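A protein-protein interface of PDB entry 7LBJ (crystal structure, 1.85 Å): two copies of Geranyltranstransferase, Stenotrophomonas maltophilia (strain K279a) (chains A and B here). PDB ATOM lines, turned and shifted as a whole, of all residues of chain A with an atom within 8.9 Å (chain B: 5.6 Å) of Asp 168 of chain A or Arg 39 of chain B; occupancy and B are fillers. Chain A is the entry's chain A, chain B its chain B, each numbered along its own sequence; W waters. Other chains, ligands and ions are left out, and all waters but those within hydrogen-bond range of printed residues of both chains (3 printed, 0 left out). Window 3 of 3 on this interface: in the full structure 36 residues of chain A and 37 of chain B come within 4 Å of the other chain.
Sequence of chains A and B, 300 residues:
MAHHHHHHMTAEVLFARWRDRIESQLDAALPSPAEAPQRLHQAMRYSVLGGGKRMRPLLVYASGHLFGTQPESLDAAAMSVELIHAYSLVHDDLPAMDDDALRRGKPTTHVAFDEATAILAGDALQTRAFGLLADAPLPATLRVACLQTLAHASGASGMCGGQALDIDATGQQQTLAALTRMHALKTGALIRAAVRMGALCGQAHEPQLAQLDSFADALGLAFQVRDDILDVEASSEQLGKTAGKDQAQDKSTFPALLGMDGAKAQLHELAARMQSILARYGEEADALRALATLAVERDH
Of the printed residues of chain B, Gly 161 of chain A touches Pro 37 (3.7 Å). Of the printed residues of chain B, Ala 164 of chain A touches Pro 37 (3.96 Å) and Leu 40 (3.8 Å). Of the printed residues of chain B, Leu 165 of chain A touches Pro 37. Of the printed residues of chain B, Asp 168 of chain A touches Arg 39 (3.98 Å). Printed residues of chain A within 4 Å of Pro 37 of chain B: Gly 161, Ala 164 and Leu 165. Gln 38 of chain B touches none of the printed residues of chain A. Of the printed residues of chain A, Arg 39 of chain B touches Asp 168. Of the printed residues of chain A, Leu 40 of chain B touches Ala 164 (3.8 Å). Asp 114 of chain B touches none of the printed residues of chain A. The nearest printed residue of chain A that does not touch Leu 40 of chain B is Gly 161 of chain A (4.002 Å).
Water W1 lies within hydrogen-bond range of OD2 of Asp 168 of chain A (2.6 Å), N of Arg 39 of chain B (2.9 Å) and N of Gln 38 of chain B (3.3 Å). Water W2 lies within hydrogen-bond range of OD2 of Asp 168 of chain A (2.8 Å) and N of Leu 40 of chain B (2.9 Å). Water W3 bridges OG1 of Thr 117 of chain B (2.8 Å) and OD1 of Asp 168 of chain A (3.2 Å).
No position is printed for both chains. Of the 5 pairs that touch across the chains among the printed residues, none has its exchanged pair printed and touching as well.
O of Pro 37 of chain B sits close to ND1 of His 41 of chain B (3.3 Å). The guanidinium group of Arg 39 of chain B sits close to the backbone carbonyl oxygen of Phe 113 of chain B, at 3.2 Å. OD2 of Asp 114 of chain B lies within salt-bridge range of NH2 of Arg 39 of chain B (2.7 Å). The guanidinium group (NE) of Arg 39 of chain B lies within hydrogen-bond range of the side-chain hydroxyl (OG1) of Thr 117 of chain B (3.4 Å).
CG of Pro 37 of chain B touches O of Gly 161 of chain A, at 3.7 Å. Ala 164 of chain A touches Pro 37 of chain B. CB of Leu 40 of chain B touches CB of Ala 164 of chain A, at 3.8 Å. Pro 37 of chain B touches Leu 165 of chain A (CB to CD2, 3.8 Å). OD1 of Asp 168 of chain A touches CD of Arg 39 of chain B, 3.98 Å away.
Hydrophobic or aromatic side chains of chain B within 4 Å of the printed part of chain A: Pro 37 and Leu 40. Hydrophobic or aromatic side chains of chain A that line the printed part of chain B: Ala 164 and Leu 165. Along chain A the printed residues that touch a printed residue of chain B span positions 161 to 168.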
ATOM      1  N   CYS A 160     -14.498  18.113 -25.173  1.00  0.00           N
ATOM      2  CA  CYS A 160     -15.942  18.228 -24.966  1.00  0.00           C
ATOM      3  C   CYS A 160     -16.487  19.527 -25.526  1.00  0.00           C
ATOM      4  O   CYS A 160     -17.568  19.544 -26.133  1.00  0.00           O
ATOM      5  CB  CYS A 160     -16.296  18.158 -23.486  1.00  0.00           C
ATOM      6  SG  CYS A 160     -16.329  16.511 -22.851  1.00  0.00           S
ATOM      7  N   GLY A 161     -15.785  20.636 -25.289  1.00  0.00           N
ATOM      8  CA  GLY A 161     -16.230  21.907 -25.854  1.00  0.00           C
ATOM      9  C   GLY A 161     -16.283  21.869 -27.370  1.00  0.00           C
ATOM     10  O   GLY A 161     -17.204  22.415 -27.990  1.00  0.00           O
ATOM     11  N   GLY A 162     -15.296  21.223 -27.989  1.00  0.00           N
ATOM     12  CA  GLY A 162     -15.290  21.130 -29.440  1.00  0.00           C
ATOM     13  C   GLY A 162     -16.420  20.271 -29.966  1.00  0.00           C
ATOM     14  O   GLY A 162     -17.042  20.606 -30.984  1.00  0.00           O
ATOM     15  N   GLN A 163     -16.702  19.149 -29.284  1.00  0.00           N
ATOM     16  CA  GLN A 163     -17.876  18.351 -29.630  1.00  0.00           C
ATOM     17  C   GLN A 163     -19.136  19.203 -29.570  1.00  0.00           C
ATOM     18  O   GLN A 163     -20.000  19.116 -30.450  1.00  0.00           O
ATOM     19  CB  GLN A 163     -18.012  17.148 -28.684  1.00  0.00           C
ATOM     20  CG  GLN A 163     -16.934  16.068 -28.815  1.00  0.00           C
ATOM     21  CD  GLN A 163     -17.032  14.990 -27.711  1.00  0.00           C
ATOM     22  OE1 GLN A 163     -16.607  15.205 -26.579  1.00  0.00           O
ATOM     23  NE2 GLN A 163     -17.601  13.839 -28.049  1.00  0.00           N
ATOM     24  N   ALA A 164     -19.257  20.038 -28.530  1.00  0.00           N
ATOM     25  CA  ALA A 164     -20.436  20.886 -28.389  1.00  0.00           C
ATOM     26  C   ALA A 164     -20.517  21.925 -29.502  1.00  0.00           C
ATOM     27  O   ALA A 164     -21.603  22.201 -30.022  1.00  0.00           O
ATOM     28  CB  ALA A 164     -20.425  21.575 -27.022  1.00  0.00           C
ATOM     29  N   LEU A 165     -19.392  22.553 -29.844  1.00  0.00           N
ATOM     30  CA  LEU A 165     -19.390  23.501 -30.959  1.00  0.00           C
ATOM     31  C   LEU A 165     -19.878  22.838 -32.238  1.00  0.00           C
ATOM     32  O   LEU A 165     -20.618  23.442 -33.022  1.00  0.00           O
ATOM     33  CB  LEU A 165     -17.987  24.064 -31.164  1.00  0.00           C
ATOM     34  CG  LEU A 165     -17.510  25.048 -30.094  1.00  0.00           C
ATOM     35  CD1 LEU A 165     -16.030  25.389 -30.272  1.00  0.00           C
ATOM     36  CD2 LEU A 165     -18.349  26.328 -30.120  1.00  0.00           C
ATOM     37  N   ASP A 166     -19.471  21.590 -32.456  1.00  0.00           N
ATOM     38  CA  ASP A 166     -19.895  20.841 -33.632  1.00  0.00           C
ATOM     39  C   ASP A 166     -21.403  20.579 -33.610  1.00  0.00           C
ATOM     40  O   ASP A 166     -22.096  20.765 -34.617  1.00  0.00           O
ATOM     41  CB  ASP A 166     -19.108  19.527 -33.686  1.00  0.00           C
ATOM     42  CG  ASP A 166     -19.083  18.924 -35.073  1.00  0.00           C
ATOM     43  OD1 ASP A 166     -19.752  19.471 -35.970  1.00  0.00           O
ATOM     44  OD2 ASP A 166     -18.378  17.916 -35.256  1.00  0.00           O
ATOM     45  N   ILE A 167     -21.925  20.133 -32.469  1.00  0.00           N
ATOM     46  CA  ILE A 167     -23.357  19.885 -32.358  1.00  0.00           C
ATOM     47  C   ILE A 167     -24.145  21.171 -32.554  1.00  0.00           C
ATOM     48  O   ILE A 167     -25.163  21.184 -33.252  1.00  0.00           O
ATOM     49  CB  ILE A 167     -23.674  19.227 -31.011  1.00  0.00           C
ATOM     50  CG1 ILE A 167     -23.211  17.777 -31.043  1.00  0.00           C
ATOM     51  CG2 ILE A 167     -25.163  19.342 -30.681  1.00  0.00           C
ATOM     52  CD1 ILE A 167     -23.525  17.098 -29.800  1.00  0.00           C
ATOM     53  N   ASP A 168     -23.678  22.279 -31.971  1.00  0.00           N
ATOM     54  CA  ASP A 168     -24.388  23.547 -32.152  1.00  0.00           C
ATOM     55  C   ASP A 168     -24.451  23.957 -33.624  1.00  0.00           C
ATOM     56  O   ASP A 168     -25.396  24.635 -34.043  1.00  0.00           O
ATOM     57  CB  ASP A 168     -23.719  24.659 -31.346  1.00  0.00           C
ATOM     58  CG  ASP A 168     -23.974  24.550 -29.837  1.00  0.00           C
ATOM     59  OD1 ASP A 168     -24.875  23.796 -29.411  1.00  0.00           O
ATOM     60  OD2 ASP A 168     -23.251  25.232 -29.077  1.00  0.00           O
ATOM     61  N   ALA A 169     -23.463  23.554 -34.417  1.00  0.00           N
ATOM     62  CA  ALA A 169     -23.350  23.975 -35.807  1.00  0.00           C
ATOM     63  C   ALA A 169     -24.067  23.044 -36.776  1.00  0.00           C
ATOM     64  O   ALA A 169     -24.021  23.286 -37.980  1.00  0.00           O
ATOM     65  CB  ALA A 169     -21.876  24.088 -36.196  1.00  0.00           C
ATOM     66  N   THR A 170     -24.714  21.988 -36.283  1.00  0.00           N
ATOM     67  CA  THR A 170     -25.423  21.054 -37.147  1.00  0.00           C
ATOM     68  C   THR A 170     -26.469  21.800 -37.965  1.00  0.00           C
ATOM     69  O   THR A 170     -27.309  22.512 -37.411  1.00  0.00           O
ATOM     70  CB  THR A 170     -26.083  19.964 -36.301  1.00  0.00           C
ATOM     71  OG1 THR A 170     -25.076  19.199 -35.621  1.00  0.00           O
ATOM     72  CG2 THR A 170     -26.915  19.039 -37.167  1.00  0.00           C
ATOM     73  N   GLY A 171     -26.402  21.663 -39.288  1.00  0.00           N
ATOM     74  CA  GLY A 171     -27.321  22.363 -40.162  1.00  0.00           C
ATOM     75  C   GLY A 171     -26.974  23.808 -40.461  1.00  0.00           C
ATOM     76  O   GLY A 171     -27.766  24.487 -41.129  1.00  0.00           O
ATOM     77  N   GLN A 172     -25.831  24.307 -39.992  1.00  0.00           N
ATOM     78  CA  GLN A 172     -25.358  25.648 -40.311  1.00  0.00           C
ATOM     79  C   GLN A 172     -24.012  25.554 -41.021  1.00  0.00           C
ATOM     80  O   GLN A 172     -23.331  24.527 -40.967  1.00  0.00           O
ATOM     81  CB  GLN A 172     -25.239  26.519 -39.047  1.00  0.00           C
ATOM     82  N   GLN A 173     -23.637  26.635 -41.705  1.00  0.00           N
ATOM     83  CA  GLN A 173     -22.386  26.706 -42.458  1.00  0.00           C
ATOM     84  C   GLN A 173     -21.394  27.543 -41.656  1.00  0.00           C
ATOM     85  O   GLN A 173     -21.572  28.754 -41.508  1.00  0.00           O
ATOM     86  CB  GLN A 173     -22.614  27.309 -43.847  1.00  0.00           C
ATOM     87  N   GLN A 174     -20.352  26.902 -41.141  1.00  0.00           N
ATOM     88  CA  GLN A 174     -19.367  27.590 -40.321  1.00  0.00           C
ATOM     89  C   GLN A 174     -18.397  28.392 -41.184  1.00  0.00           C
ATOM     90  O   GLN A 174     -18.093  28.021 -42.320  1.00  0.00           O
ATOM     91  CB  GLN A 174     -18.592  26.573 -39.473  1.00  0.00           C
ATOM     92  CG  GLN A 174     -19.487  25.790 -38.522  1.00  0.00           C
ATOM     93  CD  GLN A 174     -18.767  24.648 -37.838  1.00  0.00           C
ATOM     94  OE1 GLN A 174     -18.710  23.530 -38.362  1.00  0.00           O
ATOM     95  NE2 GLN A 174     -18.223  24.915 -36.653  1.00  0.00           N
ATOM     96  N   MET A 182     -13.233  25.191 -33.847  1.00  0.00           N
ATOM     97  CA  MET A 182     -13.908  23.961 -33.436  1.00  0.00           C
ATOM     98  C   MET A 182     -12.952  22.774 -33.471  1.00  0.00           C
ATOM     99  O   MET A 182     -12.852  22.007 -32.504  1.00  0.00           O
ATOM    100  CB  MET A 182     -15.127  23.698 -34.327  1.00  0.00           C
ATOM    101  CG  MET A 182     -15.841  22.365 -34.024  1.00  0.00           C
ATOM    102  SD  MET A 182     -16.923  21.739 -35.341  1.00  0.00           S
ATOM    103  CE  MET A 182     -15.720  21.014 -36.457  1.00  0.00           C
ATOM    104  N   ASP A 250     -22.428  19.134 -40.110  1.00  0.00           N
ATOM    105  CA  ASP A 250     -21.050  19.419 -40.500  1.00  0.00           C
ATOM    106  C   ASP A 250     -20.922  19.652 -42.011  1.00  0.00           C
ATOM    107  O   ASP A 250     -20.092  19.032 -42.680  1.00  0.00           O
ATOM    108  CB  ASP A 250     -20.126  18.278 -40.058  1.00  0.00           C
ATOM    109  N   GLU B  35     -19.834  32.516 -22.391  1.00  0.00           N
ATOM    110  CA  GLU B  35     -18.659  32.178 -23.178  1.00  0.00           C
ATOM    111  C   GLU B  35     -18.884  30.884 -23.950  1.00  0.00           C
ATOM    112  O   GLU B  35     -19.660  30.022 -23.541  1.00  0.00           O
ATOM    113  CB  GLU B  35     -17.425  32.072 -22.279  1.00  0.00           C
ATOM    114  CG  GLU B  35     -17.062  33.414 -21.624  1.00  0.00           C
ATOM    115  CD  GLU B  35     -15.831  33.333 -20.733  1.00  0.00           C
ATOM    116  OE1 GLU B  35     -15.288  32.222 -20.575  1.00  0.00           O
ATOM    117  OE2 GLU B  35     -15.406  34.380 -20.195  1.00  0.00           O
ATOM    118  N   PRO B  37     -18.316  27.219 -25.704  1.00  0.00           N
ATOM    119  CA  PRO B  37     -19.673  27.001 -26.244  1.00  0.00           C
ATOM    120  C   PRO B  37     -20.739  27.289 -25.164  1.00  0.00           C
ATOM    121  O   PRO B  37     -20.728  26.664 -24.090  1.00  0.00           O
ATOM    122  CB  PRO B  37     -19.663  25.516 -26.643  1.00  0.00           C
ATOM    123  CG  PRO B  37     -18.712  24.881 -25.673  1.00  0.00           C
ATOM    124  CD  PRO B  37     -17.656  25.947 -25.340  1.00  0.00           C
ATOM    125  N   GLN B  38     -21.628  28.243 -25.457  1.00  0.00           N
ATOM    126  CA  GLN B  38     -22.540  28.765 -24.441  1.00  0.00           C
ATOM    127  C   GLN B  38     -23.500  27.696 -23.951  1.00  0.00           C
ATOM    128  O   GLN B  38     -23.739  27.563 -22.741  1.00  0.00           O
ATOM    129  CB  GLN B  38     -23.324  29.953 -24.996  1.00  0.00           C
ATOM    130  CG  GLN B  38     -22.527  31.242 -25.122  1.00  0.00           C
ATOM    131  CD  GLN B  38     -21.664  31.325 -26.374  1.00  0.00           C
ATOM    132  OE1 GLN B  38     -21.779  30.511 -27.291  1.00  0.00           O
ATOM    133  NE2 GLN B  38     -20.794  32.329 -26.417  1.00  0.00           N
ATOM    134  N   ARG B  39     -24.091  26.934 -24.871  1.00  0.00           N
ATOM    135  CA  ARG B  39     -25.150  26.023 -24.447  1.00  0.00           C
ATOM    136  C   ARG B  39     -24.596  24.922 -23.552  1.00  0.00           C
ATOM    137  O   ARG B  39     -25.232  24.538 -22.562  1.00  0.00           O
ATOM    138  CB  ARG B  39     -25.858  25.441 -25.669  1.00  0.00           C
ATOM    139  CG  ARG B  39     -27.094  24.595 -25.372  1.00  0.00           C
ATOM    140  CD  ARG B  39     -27.749  24.160 -26.679  1.00  0.00           C
ATOM    141  NE  ARG B  39     -28.891  23.270 -26.508  1.00  0.00           N
ATOM    142  CZ  ARG B  39     -30.139  23.671 -26.313  1.00  0.00           C
ATOM    143  NH1 ARG B  39     -30.435  24.949 -26.143  1.00  0.00           N
ATOM    144  NH2 ARG B  39     -31.114  22.767 -26.287  1.00  0.00           N
ATOM    145  N   LEU B  40     -23.399  24.419 -23.862  1.00  0.00           N
ATOM    146  CA  LEU B  40     -22.782  23.422 -22.979  1.00  0.00           C
ATOM    147  C   LEU B  40     -22.547  23.991 -21.582  1.00  0.00           C
ATOM    148  O   LEU B  40     -22.866  23.349 -20.570  1.00  0.00           O
ATOM    149  CB  LEU B  40     -21.463  22.947 -23.583  1.00  0.00           C
ATOM    150  CG  LEU B  40     -20.642  22.042 -22.654  1.00  0.00           C
ATOM    151  CD1 LEU B  40     -21.382  20.758 -22.446  1.00  0.00           C
ATOM    152  CD2 LEU B  40     -19.288  21.791 -23.275  1.00  0.00           C
ATOM    153  N   HIS B  41     -21.971  25.191 -21.510  1.00  0.00           N
ATOM    154  CA  HIS B  41     -21.712  25.816 -20.214  1.00  0.00           C
ATOM    155  C   HIS B  41     -22.998  26.024 -19.428  1.00  0.00           C
ATOM    156  O   HIS B  41     -23.027  25.826 -18.201  1.00  0.00           O
ATOM    157  CB  HIS B  41     -20.999  27.156 -20.413  1.00  0.00           C
ATOM    158  CG  HIS B  41     -19.641  27.036 -21.028  1.00  0.00           C
ATOM    159  ND1 HIS B  41     -19.023  28.082 -21.680  1.00  0.00           N
ATOM    160  CD2 HIS B  41     -18.775  25.995 -21.078  1.00  0.00           C
ATOM    161  CE1 HIS B  41     -17.838  27.686 -22.117  1.00  0.00           C
ATOM    162  NE2 HIS B  41     -17.666  26.423 -21.767  1.00  0.00           N
ATOM    163  N   GLN B  42     -24.060  26.464 -20.103  1.00  0.00           N
ATOM    164  CA  GLN B  42     -25.337  26.663 -19.429  1.00  0.00           C
ATOM    165  C   GLN B  42     -25.875  25.343 -18.896  1.00  0.00           C
ATOM    166  O   GLN B  42     -26.398  25.284 -17.777  1.00  0.00           O
ATOM    167  CB  GLN B  42     -26.341  27.294 -20.388  1.00  0.00           C
ATOM    168  CG  GLN B  42     -25.947  28.704 -20.759  1.00  0.00           C
ATOM    169  CD  GLN B  42     -26.507  29.141 -22.094  1.00  0.00           C
ATOM    170  OE1 GLN B  42     -27.446  28.538 -22.617  1.00  0.00           O
ATOM    171  NE2 GLN B  42     -25.935  30.203 -22.649  1.00  0.00           N
ATOM    172  N   ALA B  43     -25.745  24.267 -19.682  1.00  0.00           N
ATOM    173  CA  ALA B  43     -26.249  22.971 -19.219  1.00  0.00           C
ATOM    174  C   ALA B  43     -25.396  22.430 -18.079  1.00  0.00           C
ATOM    175  O   ALA B  43     -25.916  21.777 -17.159  1.00  0.00           O
ATOM    176  CB  ALA B  43     -26.301  21.981 -20.379  1.00  0.00           C
ATOM    177  N   MET B  44     -24.071  22.642 -18.142  1.00  0.00           N
ATOM    178  CA  MET B  44     -23.223  22.245 -17.015  1.00  0.00           C
ATOM    179  C   MET B  44     -23.665  22.947 -15.743  1.00  0.00           C
ATOM    180  O   MET B  44     -23.814  22.310 -14.695  1.00  0.00           O
ATOM    181  CB  MET B  44     -21.748  22.550 -17.291  1.00  0.00           C
ATOM    182  CG  MET B  44     -21.083  21.634 -18.337  1.00  0.00           C
ATOM    183  SD  MET B  44     -19.527  22.308 -18.924  1.00  0.00           S
ATOM    184  CE  MET B  44     -18.404  21.977 -17.575  1.00  0.00           C
ATOM    185  N   ALA B 112     -34.522  20.431 -20.297  1.00  0.00           N
ATOM    186  CA  ALA B 112     -34.263  21.872 -20.337  1.00  0.00           C
ATOM    187  C   ALA B 112     -33.414  22.255 -21.544  1.00  0.00           C
ATOM    188  O   ALA B 112     -33.490  23.394 -22.039  1.00  0.00           O
ATOM    189  CB  ALA B 112     -33.563  22.298 -19.039  1.00  0.00           C
ATOM    190  N   PHE B 113     -32.581  21.327 -22.005  1.00  0.00           N
ATOM    191  CA  PHE B 113     -31.708  21.552 -23.144  1.00  0.00           C
ATOM    192  C   PHE B 113     -32.073  20.532 -24.210  1.00  0.00           C
ATOM    193  O   PHE B 113     -33.119  20.667 -24.851  1.00  0.00           O
ATOM    194  CB  PHE B 113     -30.237  21.484 -22.694  1.00  0.00           C
ATOM    195  CG  PHE B 113     -29.863  22.624 -21.793  1.00  0.00           C
ATOM    196  CD1 PHE B 113     -30.116  22.552 -20.419  1.00  0.00           C
ATOM    197  CD2 PHE B 113     -29.345  23.807 -22.326  1.00  0.00           C
ATOM    198  CE1 PHE B 113     -29.816  23.625 -19.601  1.00  0.00           C
ATOM    199  CE2 PHE B 113     -29.034  24.890 -21.505  1.00  0.00           C
ATOM    200  CZ  PHE B 113     -29.284  24.804 -20.142  1.00  0.00           C
ATOM    201  N   ASP B 114     -31.235  19.511 -24.402  1.00  0.00           N
ATOM    202  CA  ASP B 114     -31.558  18.402 -25.292  1.00  0.00           C
ATOM    203  C   ASP B 114     -30.644  17.237 -24.925  1.00  0.00           C
ATOM    204  O   ASP B 114     -29.736  17.378 -24.107  1.00  0.00           O
ATOM    205  CB  ASP B 114     -31.388  18.801 -26.761  1.00  0.00           C
ATOM    206  CG  ASP B 114     -30.016  19.377 -27.041  1.00  0.00           C
ATOM    207  OD1 ASP B 114     -29.028  18.630 -26.959  1.00  0.00           O
ATOM    208  OD2 ASP B 114     -29.922  20.583 -27.338  1.00  0.00           O
ATOM    209  N   THR B 117     -26.735  17.720 -25.683  1.00  0.00           N
ATOM    210  CA  THR B 117     -26.156  18.665 -24.733  1.00  0.00           C
ATOM    211  C   THR B 117     -26.031  18.056 -23.338  1.00  0.00           C
ATOM    212  O   THR B 117     -25.031  18.284 -22.644  1.00  0.00           O
ATOM    213  CB  THR B 117     -26.996  19.953 -24.700  1.00  0.00           C
ATOM    214  OG1 THR B 117     -26.987  20.553 -26.002  1.00  0.00           O
ATOM    215  CG2 THR B 117     -26.406  20.967 -23.722  1.00  0.00           C
HETATM  216  O   HOH W   1     -23.931  27.367 -27.718  1.00  0.00           O
HETATM  217  O   HOH W   2     -22.817  23.968 -26.644  1.00  0.00           O
HETATM  218  O   HOH W   3     -24.619  21.746 -27.018  1.00  0.00           O
